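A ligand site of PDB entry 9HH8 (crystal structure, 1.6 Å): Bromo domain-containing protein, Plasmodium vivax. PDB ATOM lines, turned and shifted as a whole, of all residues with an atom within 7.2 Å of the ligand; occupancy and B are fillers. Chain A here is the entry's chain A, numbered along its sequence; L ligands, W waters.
A nitrogen (N1) of the ligand is in hydrogen-bond range of the backbone carbonyl oxygen of Ile 25 (2.7 Å). ND2 of Asn 83 lies within hydrogen-bond range of O2 of the ligand.
O of Cys 79 sits at hydrogen-bond distance from ND2 of Asn 83 (2.9 Å). The backbone carbonyl oxygen (O) of Gln 35 is in hydrogen-bond range of the side-chain sulfur (SG) of Cys 37 (3.7 Å). OE1 of Gln 35 sits at hydrogen-bond distance from N of Asp 31, at 2.8 Å. SG of Cys 79 lies within hydrogen-bond range of O of Val 89 (3.5 Å).
Merely in contact with the ligand: Val 30, Tyr 82, Gln 35, Phe 26, Tyr 40 and Val 89. Hydrophobic or aromatic side chains within 4 Å of the ligand: Ile 25, Phe 26, Val 30, Tyr 40, Tyr 82 and Val 89. Within 4 Å of the ligand: Ile 25, Phe 26, Val 30, Gln 35, Tyr 40, Tyr 82, Asn 83 and Val 89. The nearest printed residue that does not touch the ligand is His 24 (4.02 Å).
Water W4 bridges the side-chain hydroxyl of Tyr 40 (2.7 Å) and an oxygen (O2) of the ligand (2.7 Å).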
ATOM      1  N   HIS A  24      22.052  -2.247 -19.446  1.00  0.00           N
ATOM      2  CA  HIS A  24      20.929  -1.552 -18.833  1.00  0.00           C
ATOM      3  C   HIS A  24      19.886  -1.140 -19.861  1.00  0.00           C
ATOM      4  O   HIS A  24      18.722  -0.953 -19.503  1.00  0.00           O
ATOM      5  CB  HIS A  24      21.410  -0.331 -18.034  1.00  0.00           C
ATOM      6  CG  HIS A  24      22.035   0.720 -18.895  1.00  0.00           C
ATOM      7  ND1 HIS A  24      23.361   0.658 -19.285  1.00  0.00           N
ATOM      8  CD2 HIS A  24      21.522   1.845 -19.453  1.00  0.00           C
ATOM      9  CE1 HIS A  24      23.640   1.707 -20.065  1.00  0.00           C
ATOM     10  NE2 HIS A  24      22.548   2.452 -20.176  1.00  0.00           N
ATOM     11  N   ILE A  25      20.276  -0.926 -21.136  1.00  0.00           N
ATOM     12  CA  ILE A  25      19.256  -0.500 -22.075  1.00  0.00           C
ATOM     13  C   ILE A  25      18.268  -1.586 -22.453  1.00  0.00           C
ATOM     14  O   ILE A  25      17.203  -1.247 -22.966  1.00  0.00           O
ATOM     15  CB  ILE A  25      19.914   0.023 -23.373  1.00  0.00           C
ATOM     16  CG1 ILE A  25      20.462  -1.116 -24.217  1.00  0.00           C
ATOM     17  CG2 ILE A  25      20.966   1.109 -22.997  1.00  0.00           C
ATOM     18  CD1 ILE A  25      21.006  -0.512 -25.625  1.00  0.00           C
ATOM     19  N   PHE A  26      18.526  -2.843 -22.071  1.00  0.00           N
ATOM     20  CA  PHE A  26      17.609  -3.950 -22.340  1.00  0.00           C
ATOM     21  C   PHE A  26      16.926  -4.392 -21.075  1.00  0.00           C
ATOM     22  O   PHE A  26      16.095  -5.324 -21.145  1.00  0.00           O
ATOM     23  CB  PHE A  26      18.347  -5.121 -22.969  1.00  0.00           C
ATOM     24  CG  PHE A  26      19.011  -4.770 -24.289  1.00  0.00           C
ATOM     25  CD1 PHE A  26      18.230  -4.412 -25.353  1.00  0.00           C
ATOM     26  CD2 PHE A  26      20.372  -4.865 -24.417  1.00  0.00           C
ATOM     27  CE1 PHE A  26      18.813  -4.082 -26.599  1.00  0.00           C
ATOM     28  CE2 PHE A  26      21.000  -4.495 -25.687  1.00  0.00           C
ATOM     29  CZ  PHE A  26      20.206  -4.089 -26.743  1.00  0.00           C
ATOM     30  N   GLU A  27      17.217  -3.737 -19.944  1.00  0.00           N
ATOM     31  CA  GLU A  27      16.746  -4.280 -18.651  1.00  0.00           C
ATOM     32  C   GLU A  27      15.243  -4.188 -18.528  1.00  0.00           C
ATOM     33  O   GLU A  27      14.577  -5.149 -18.091  1.00  0.00           O
ATOM     34  CB  GLU A  27      17.460  -3.572 -17.495  1.00  0.00           C
ATOM     35  CG  GLU A  27      17.087  -4.248 -16.099  1.00  0.00           C
ATOM     36  CD  GLU A  27      17.650  -5.621 -15.962  1.00  0.00           C
ATOM     37  OE1 GLU A  27      18.697  -5.926 -16.581  1.00  0.00           O
ATOM     38  OE2 GLU A  27      17.009  -6.467 -15.250  1.00  0.00           O
ATOM     39  N   LYS A  28      14.699  -3.003 -18.767  1.00  0.00           N
ATOM     40  CA  LYS A  28      13.263  -2.727 -18.725  1.00  0.00           C
ATOM     41  C   LYS A  28      12.697  -2.536 -20.109  1.00  0.00           C
ATOM     42  O   LYS A  28      13.438  -2.180 -21.060  1.00  0.00           O
ATOM     43  CB  LYS A  28      12.957  -1.474 -17.904  1.00  0.00           C
ATOM     44  CG  LYS A  28      13.529  -1.464 -16.510  1.00  0.00           C
ATOM     45  CD  LYS A  28      12.991  -2.681 -15.754  1.00  0.00           C
ATOM     46  CE  LYS A  28      13.342  -2.530 -14.270  1.00  0.00           C
ATOM     47  NZ  LYS A  28      12.965  -3.703 -13.441  1.00  0.00           N
ATOM     48  N   LEU A  29      11.372  -2.639 -20.222  1.00  0.00           N
ATOM     49  CA  LEU A  29      10.724  -2.325 -21.499  1.00  0.00           C
ATOM     50  C   LEU A  29      10.868  -0.845 -21.814  1.00  0.00           C
ATOM     51  O   LEU A  29      10.904   0.018 -20.934  1.00  0.00           O
ATOM     52  CB  LEU A  29       9.239  -2.712 -21.483  1.00  0.00           C
ATOM     53  CG  LEU A  29       9.032  -4.225 -21.415  1.00  0.00           C
ATOM     54  CD1 LEU A  29       7.642  -4.455 -20.819  1.00  0.00           C
ATOM     55  CD2 LEU A  29       9.184  -4.851 -22.792  1.00  0.00           C
ATOM     56  N   VAL A  30      10.991  -0.551 -23.104  1.00  0.00           N
ATOM     57  CA  VAL A  30      11.194   0.824 -23.546  1.00  0.00           C
ATOM     58  C   VAL A  30       9.966   1.659 -23.196  1.00  0.00           C
ATOM     59  O   VAL A  30       8.824   1.237 -23.441  1.00  0.00           O
ATOM     60  CB  VAL A  30      11.443   0.824 -25.066  1.00  0.00           C
ATOM     61  CG1 VAL A  30      11.466   2.244 -25.585  1.00  0.00           C
ATOM     62  CG2 VAL A  30      12.711   0.088 -25.372  1.00  0.00           C
ATOM     63  N   ASP A  31      10.181   2.829 -22.628  1.00  0.00           N
ATOM     64  CA  ASP A  31       9.108   3.813 -22.410  1.00  0.00           C
ATOM     65  C   ASP A  31       9.043   4.743 -23.624  1.00  0.00           C
ATOM     66  O   ASP A  31       9.963   5.559 -23.842  1.00  0.00           O
ATOM     67  CB  ASP A  31       9.386   4.566 -21.112  1.00  0.00           C
ATOM     68  CG  ASP A  31       8.268   5.509 -20.721  1.00  0.00           C
ATOM     69  OD1 ASP A  31       7.719   6.246 -21.580  1.00  0.00           O
ATOM     70  OD2 ASP A  31       7.924   5.533 -19.530  1.00  0.00           O
ATOM     71  N   LYS A  34       9.352   8.518 -22.791  1.00  0.00           N
ATOM     72  CA  LYS A  34      10.538   8.902 -22.046  1.00  0.00           C
ATOM     73  C   LYS A  34      11.824   8.688 -22.868  1.00  0.00           C
ATOM     74  O   LYS A  34      12.775   9.466 -22.744  1.00  0.00           O
ATOM     75  CB  LYS A  34      10.581   8.138 -20.709  1.00  0.00           C
ATOM     76  CG  LYS A  34      11.853   8.293 -19.915  1.00  0.00           C
ATOM     77  N   GLN A  35      11.866   7.666 -23.702  1.00  0.00           N
ATOM     78  CA  GLN A  35      13.011   7.419 -24.558  1.00  0.00           C
ATOM     79  C   GLN A  35      12.878   8.099 -25.928  1.00  0.00           C
ATOM     80  O   GLN A  35      13.644   7.790 -26.829  1.00  0.00           O
ATOM     81  CB  GLN A  35      13.234   5.886 -24.692  1.00  0.00           C
ATOM     82  CG  GLN A  35      14.117   5.237 -23.577  1.00  0.00           C
ATOM     83  CD  GLN A  35      13.415   5.033 -22.213  1.00  0.00           C
ATOM     84  OE1 GLN A  35      12.601   4.107 -22.014  1.00  0.00           O
ATOM     85  NE2 GLN A  35      13.771   5.867 -21.253  1.00  0.00           N
ATOM     86  N   ASN A  36      11.896   8.984 -26.089  1.00  0.00           N
ATOM     87  CA  ASN A  36      11.730   9.803 -27.295  1.00  0.00           C
ATOM     88  C   ASN A  36      11.606   8.970 -28.553  1.00  0.00           C
ATOM     89  O   ASN A  36      12.156   9.276 -29.617  1.00  0.00           O
ATOM     90  CB  ASN A  36      12.877  10.828 -27.440  1.00  0.00           C
ATOM     91  CG  ASN A  36      12.832  11.833 -26.344  1.00  0.00           C
ATOM     92  OD1 ASN A  36      11.865  12.609 -26.270  1.00  0.00           O
ATOM     93  ND2 ASN A  36      13.828  11.830 -25.454  1.00  0.00           N
ATOM     94  N   CYS A  37      10.857   7.884 -28.458  1.00  0.00           N
ATOM     95  CA  CYS A  37      10.629   7.001 -29.591  1.00  0.00           C
ATOM     96  C   CYS A  37       9.141   6.674 -29.648  1.00  0.00           C
ATOM     97  O   CYS A  37       8.718   5.535 -29.391  1.00  0.00           O
ATOM     98  CB  CYS A  37      11.518   5.753 -29.479  1.00  0.00           C
ATOM     99  SG  CYS A  37      11.461   4.945 -27.887  1.00  0.00           S
ATOM    100  N   TYR A  40       7.662   3.396 -31.179  1.00  0.00           N
ATOM    101  CA  TYR A  40       8.379   2.156 -30.882  1.00  0.00           C
ATOM    102  C   TYR A  40       7.431   0.945 -30.965  1.00  0.00           C
ATOM    103  O   TYR A  40       7.762  -0.096 -31.567  1.00  0.00           O
ATOM    104  CB  TYR A  40       9.026   2.246 -29.485  1.00  0.00           C
ATOM    105  CG  TYR A  40       9.788   1.000 -29.139  1.00  0.00           C
ATOM    106  CD1 TYR A  40      11.048   0.805 -29.620  1.00  0.00           C
ATOM    107  CD2 TYR A  40       9.215  -0.018 -28.311  1.00  0.00           C
ATOM    108  CE1 TYR A  40      11.777  -0.321 -29.370  1.00  0.00           C
ATOM    109  CE2 TYR A  40       9.906  -1.193 -28.087  1.00  0.00           C
ATOM    110  CZ  TYR A  40      11.190  -1.342 -28.561  1.00  0.00           C
ATOM    111  OH  TYR A  40      11.940  -2.459 -28.312  1.00  0.00           O
ATOM    112  N   ILE A  44       7.556  -2.494 -33.009  1.00  0.00           N
ATOM    113  CA  ILE A  44       7.885  -3.674 -32.212  1.00  0.00           C
ATOM    114  C   ILE A  44       6.597  -4.212 -31.605  1.00  0.00           C
ATOM    115  O   ILE A  44       6.020  -3.580 -30.716  1.00  0.00           O
ATOM    116  CB  ILE A  44       8.895  -3.317 -31.109  1.00  0.00           C
ATOM    117  CG1 ILE A  44      10.198  -2.794 -31.766  1.00  0.00           C
ATOM    118  CG2 ILE A  44       9.140  -4.522 -30.169  1.00  0.00           C
ATOM    119  CD1 ILE A  44      10.751  -3.750 -32.830  1.00  0.00           C
ATOM    120  N   MET A  48      10.166  -7.184 -25.417  1.00  0.00           N
ATOM    121  CA  MET A  48      10.850  -8.073 -24.485  1.00  0.00           C
ATOM    122  C   MET A  48      12.032  -7.336 -23.836  1.00  0.00           C
ATOM    123  O   MET A  48      12.759  -6.592 -24.505  1.00  0.00           O
ATOM    124  CB  MET A  48      11.337  -9.321 -25.222  1.00  0.00           C
ATOM    125  CG  MET A  48      11.791 -10.438 -24.292  1.00  0.00           C
ATOM    126  SD  MET A  48      10.484 -11.126 -23.166  1.00  0.00           S
ATOM    127  CE  MET A  48       9.321 -11.792 -24.380  1.00  0.00           C
ATOM    128  N   ILE A  75      14.759 -10.014 -27.812  1.00  0.00           N
ATOM    129  CA  ILE A  75      15.315  -8.717 -27.420  1.00  0.00           C
ATOM    130  C   ILE A  75      16.246  -8.201 -28.506  1.00  0.00           C
ATOM    131  O   ILE A  75      16.125  -7.045 -28.957  1.00  0.00           O
ATOM    132  CB  ILE A  75      16.035  -8.826 -26.065  1.00  0.00           C
ATOM    133  CG1 ILE A  75      15.044  -9.322 -25.009  1.00  0.00           C
ATOM    134  CG2 ILE A  75      16.552  -7.433 -25.657  1.00  0.00           C
ATOM    135  CD1 ILE A  75      15.645  -9.502 -23.617  1.00  0.00           C
ATOM    136  N   ASN A  78      14.430  -7.430 -31.890  1.00  0.00           N
ATOM    137  CA  ASN A  78      13.738  -6.156 -31.809  1.00  0.00           C
ATOM    138  C   ASN A  78      14.726  -4.993 -31.945  1.00  0.00           C
ATOM    139  O   ASN A  78      14.425  -4.003 -32.604  1.00  0.00           O
ATOM    140  CB  ASN A  78      12.979  -6.013 -30.489  1.00  0.00           C
ATOM    141  CG  ASN A  78      11.757  -6.924 -30.458  1.00  0.00           C
ATOM    142  OD1 ASN A  78      11.321  -7.407 -31.483  1.00  0.00           O
ATOM    143  ND2 ASN A  78      11.254  -7.169 -29.268  1.00  0.00           N
ATOM    144  N   CYS A  79      15.890  -5.108 -31.295  1.00  0.00           N
ATOM    145  CA  CYS A  79      16.901  -4.043 -31.298  1.00  0.00           C
ATOM    146  C   CYS A  79      17.359  -3.793 -32.736  1.00  0.00           C
ATOM    147  O   CYS A  79      17.438  -2.641 -33.194  1.00  0.00           O
ATOM    148  CB  CYS A  79      18.070  -4.474 -30.403  1.00  0.00           C
ATOM    149  SG  CYS A  79      19.372  -3.250 -30.342  1.00  0.00           S
ATOM    150  N   SER A  80      17.662  -4.871 -33.456  1.00  0.00           N
ATOM    151  CA  SER A  80      18.173  -4.683 -34.823  1.00  0.00           C
ATOM    152  C   SER A  80      17.095  -4.201 -35.794  1.00  0.00           C
ATOM    153  O   SER A  80      17.396  -3.450 -36.740  1.00  0.00           O
ATOM    154  CB  SER A  80      18.854  -5.973 -35.264  1.00  0.00           C
ATOM    155  OG  SER A  80      17.921  -6.987 -35.457  1.00  0.00           O
ATOM    156  N   TYR A  82      14.366  -2.117 -34.955  1.00  0.00           N
ATOM    157  CA  TYR A  82      14.001  -0.731 -34.699  1.00  0.00           C
ATOM    158  C   TYR A  82      15.174   0.213 -34.971  1.00  0.00           C
ATOM    159  O   TYR A  82      14.979   1.322 -35.488  1.00  0.00           O
ATOM    160  CB  TYR A  82      13.540  -0.531 -33.231  1.00  0.00           C
ATOM    161  CG  TYR A  82      12.994   0.865 -33.040  1.00  0.00           C
ATOM    162  CD1 TYR A  82      11.743   1.226 -33.509  1.00  0.00           C
ATOM    163  CD2 TYR A  82      13.787   1.865 -32.442  1.00  0.00           C
ATOM    164  CE1 TYR A  82      11.250   2.512 -33.384  1.00  0.00           C
ATOM    165  CE2 TYR A  82      13.322   3.154 -32.318  1.00  0.00           C
ATOM    166  CZ  TYR A  82      12.060   3.486 -32.784  1.00  0.00           C
ATOM    167  OH  TYR A  82      11.636   4.794 -32.663  1.00  0.00           O
ATOM    168  N   ASN A  83      16.384  -0.169 -34.550  1.00  0.00           N
ATOM    169  CA  ASN A  83      17.518   0.776 -34.521  1.00  0.00           C
ATOM    170  C   ASN A  83      18.376   0.663 -35.765  1.00  0.00           C
ATOM    171  O   ASN A  83      18.639  -0.432 -36.272  1.00  0.00           O
ATOM    172  CB  ASN A  83      18.377   0.536 -33.295  1.00  0.00           C
ATOM    173  CG  ASN A  83      17.589   0.723 -32.017  1.00  0.00           C
ATOM    174  OD1 ASN A  83      17.421   1.842 -31.564  1.00  0.00           O
ATOM    175  ND2 ASN A  83      17.019  -0.406 -31.464  1.00  0.00           N
ATOM    176  N   VAL A  89      22.716   2.127 -29.911  1.00  0.00           N
ATOM    177  CA  VAL A  89      21.832   1.034 -29.441  1.00  0.00           C
ATOM    178  C   VAL A  89      22.039  -0.232 -30.269  1.00  0.00           C
ATOM    179  O   VAL A  89      22.186  -1.338 -29.720  1.00  0.00           O
ATOM    180  CB  VAL A  89      20.363   1.527 -29.388  1.00  0.00           C
ATOM    181  CG1 VAL A  89      19.339   0.333 -29.189  1.00  0.00           C
ATOM    182  CG2 VAL A  89      20.186   2.508 -28.287  1.00  0.00           C
ATOM    183  N   ALA A  90      22.104  -0.126 -31.618  1.00  0.00           N
ATOM    184  CA  ALA A  90      22.289  -1.323 -32.439  1.00  0.00           C
ATOM    185  C   ALA A  90      23.622  -1.987 -32.109  1.00  0.00           C
ATOM    186  O   ALA A  90      23.728  -3.213 -32.084  1.00  0.00           O
ATOM    187  CB  ALA A  90      22.249  -0.980 -33.946  1.00  0.00           C
HETATM  188  N1  LIG L   1      16.594   0.459 -24.981  1.00  0.00           N
HETATM  189  C1  LIG L   1      16.550   1.847 -24.926  1.00  0.00           C
HETATM  190  C2  LIG L   1      16.935   2.574 -23.710  1.00  0.00           C
HETATM  191  C3  LIG L   1      18.027   3.450 -23.686  1.00  0.00           C
HETATM  192  C4  LIG L   1      18.397   4.012 -22.473  1.00  0.00           C
HETATM  193  C5  LIG L   1      17.734   3.726 -21.286  1.00  0.00           C
HETATM  194  C6  LIG L   1      16.265   2.295 -22.514  1.00  0.00           C
HETATM  195  C7  LIG L   1      16.251   0.013 -26.241  1.00  0.00           C
HETATM  196  C8  LIG L   1      15.486   1.080 -28.401  1.00  0.00           C
HETATM  197  N2  LIG L   1      17.416   3.969 -18.914  1.00  0.00           N
HETATM  198  C9  LIG L   1      15.948   3.466 -29.110  1.00  0.00           C
HETATM  199  O1  LIG L   1      19.124   5.040 -19.900  1.00  0.00           O
HETATM  200  C10 LIG L   1      16.280   4.239 -27.835  1.00  0.00           C
HETATM  201  C11 LIG L   1      18.135   4.296 -19.964  1.00  0.00           C
HETATM  202  C12 LIG L   1      18.827   3.765 -24.928  1.00  0.00           C
HETATM  203  C13 LIG L   1      15.944   1.140 -27.006  1.00  0.00           C
HETATM  204  C14 LIG L   1      15.709   3.713 -26.520  1.00  0.00           C
HETATM  205  C15 LIG L   1      16.113   2.302 -26.175  1.00  0.00           C
HETATM  206  C16 LIG L   1      16.662   2.859 -21.321  1.00  0.00           C
HETATM  207  O2  LIG L   1      15.476   0.024 -29.032  1.00  0.00           O
HETATM  208  C17 LIG L   1      14.939   2.356 -29.006  1.00  0.00           C
HETATM  209  C18 LIG L   1      16.244  -1.443 -26.573  1.00  0.00           C
HETATM  210  O   HOH W   1      15.482  -4.629 -27.689  1.00  0.00           O
HETATM  211  O   HOH W   2      13.993   0.767 -20.917  1.00  0.00           O
HETATM  212  O   HOH W   3      15.362   1.501 -17.750  1.00  0.00           O
HETATM  213  O   HOH W   4      14.476  -2.520 -29.300  1.00  0.00           O
HETATM  214  O   HOH W   5      20.692   7.533 -21.580  1.00  0.00           O
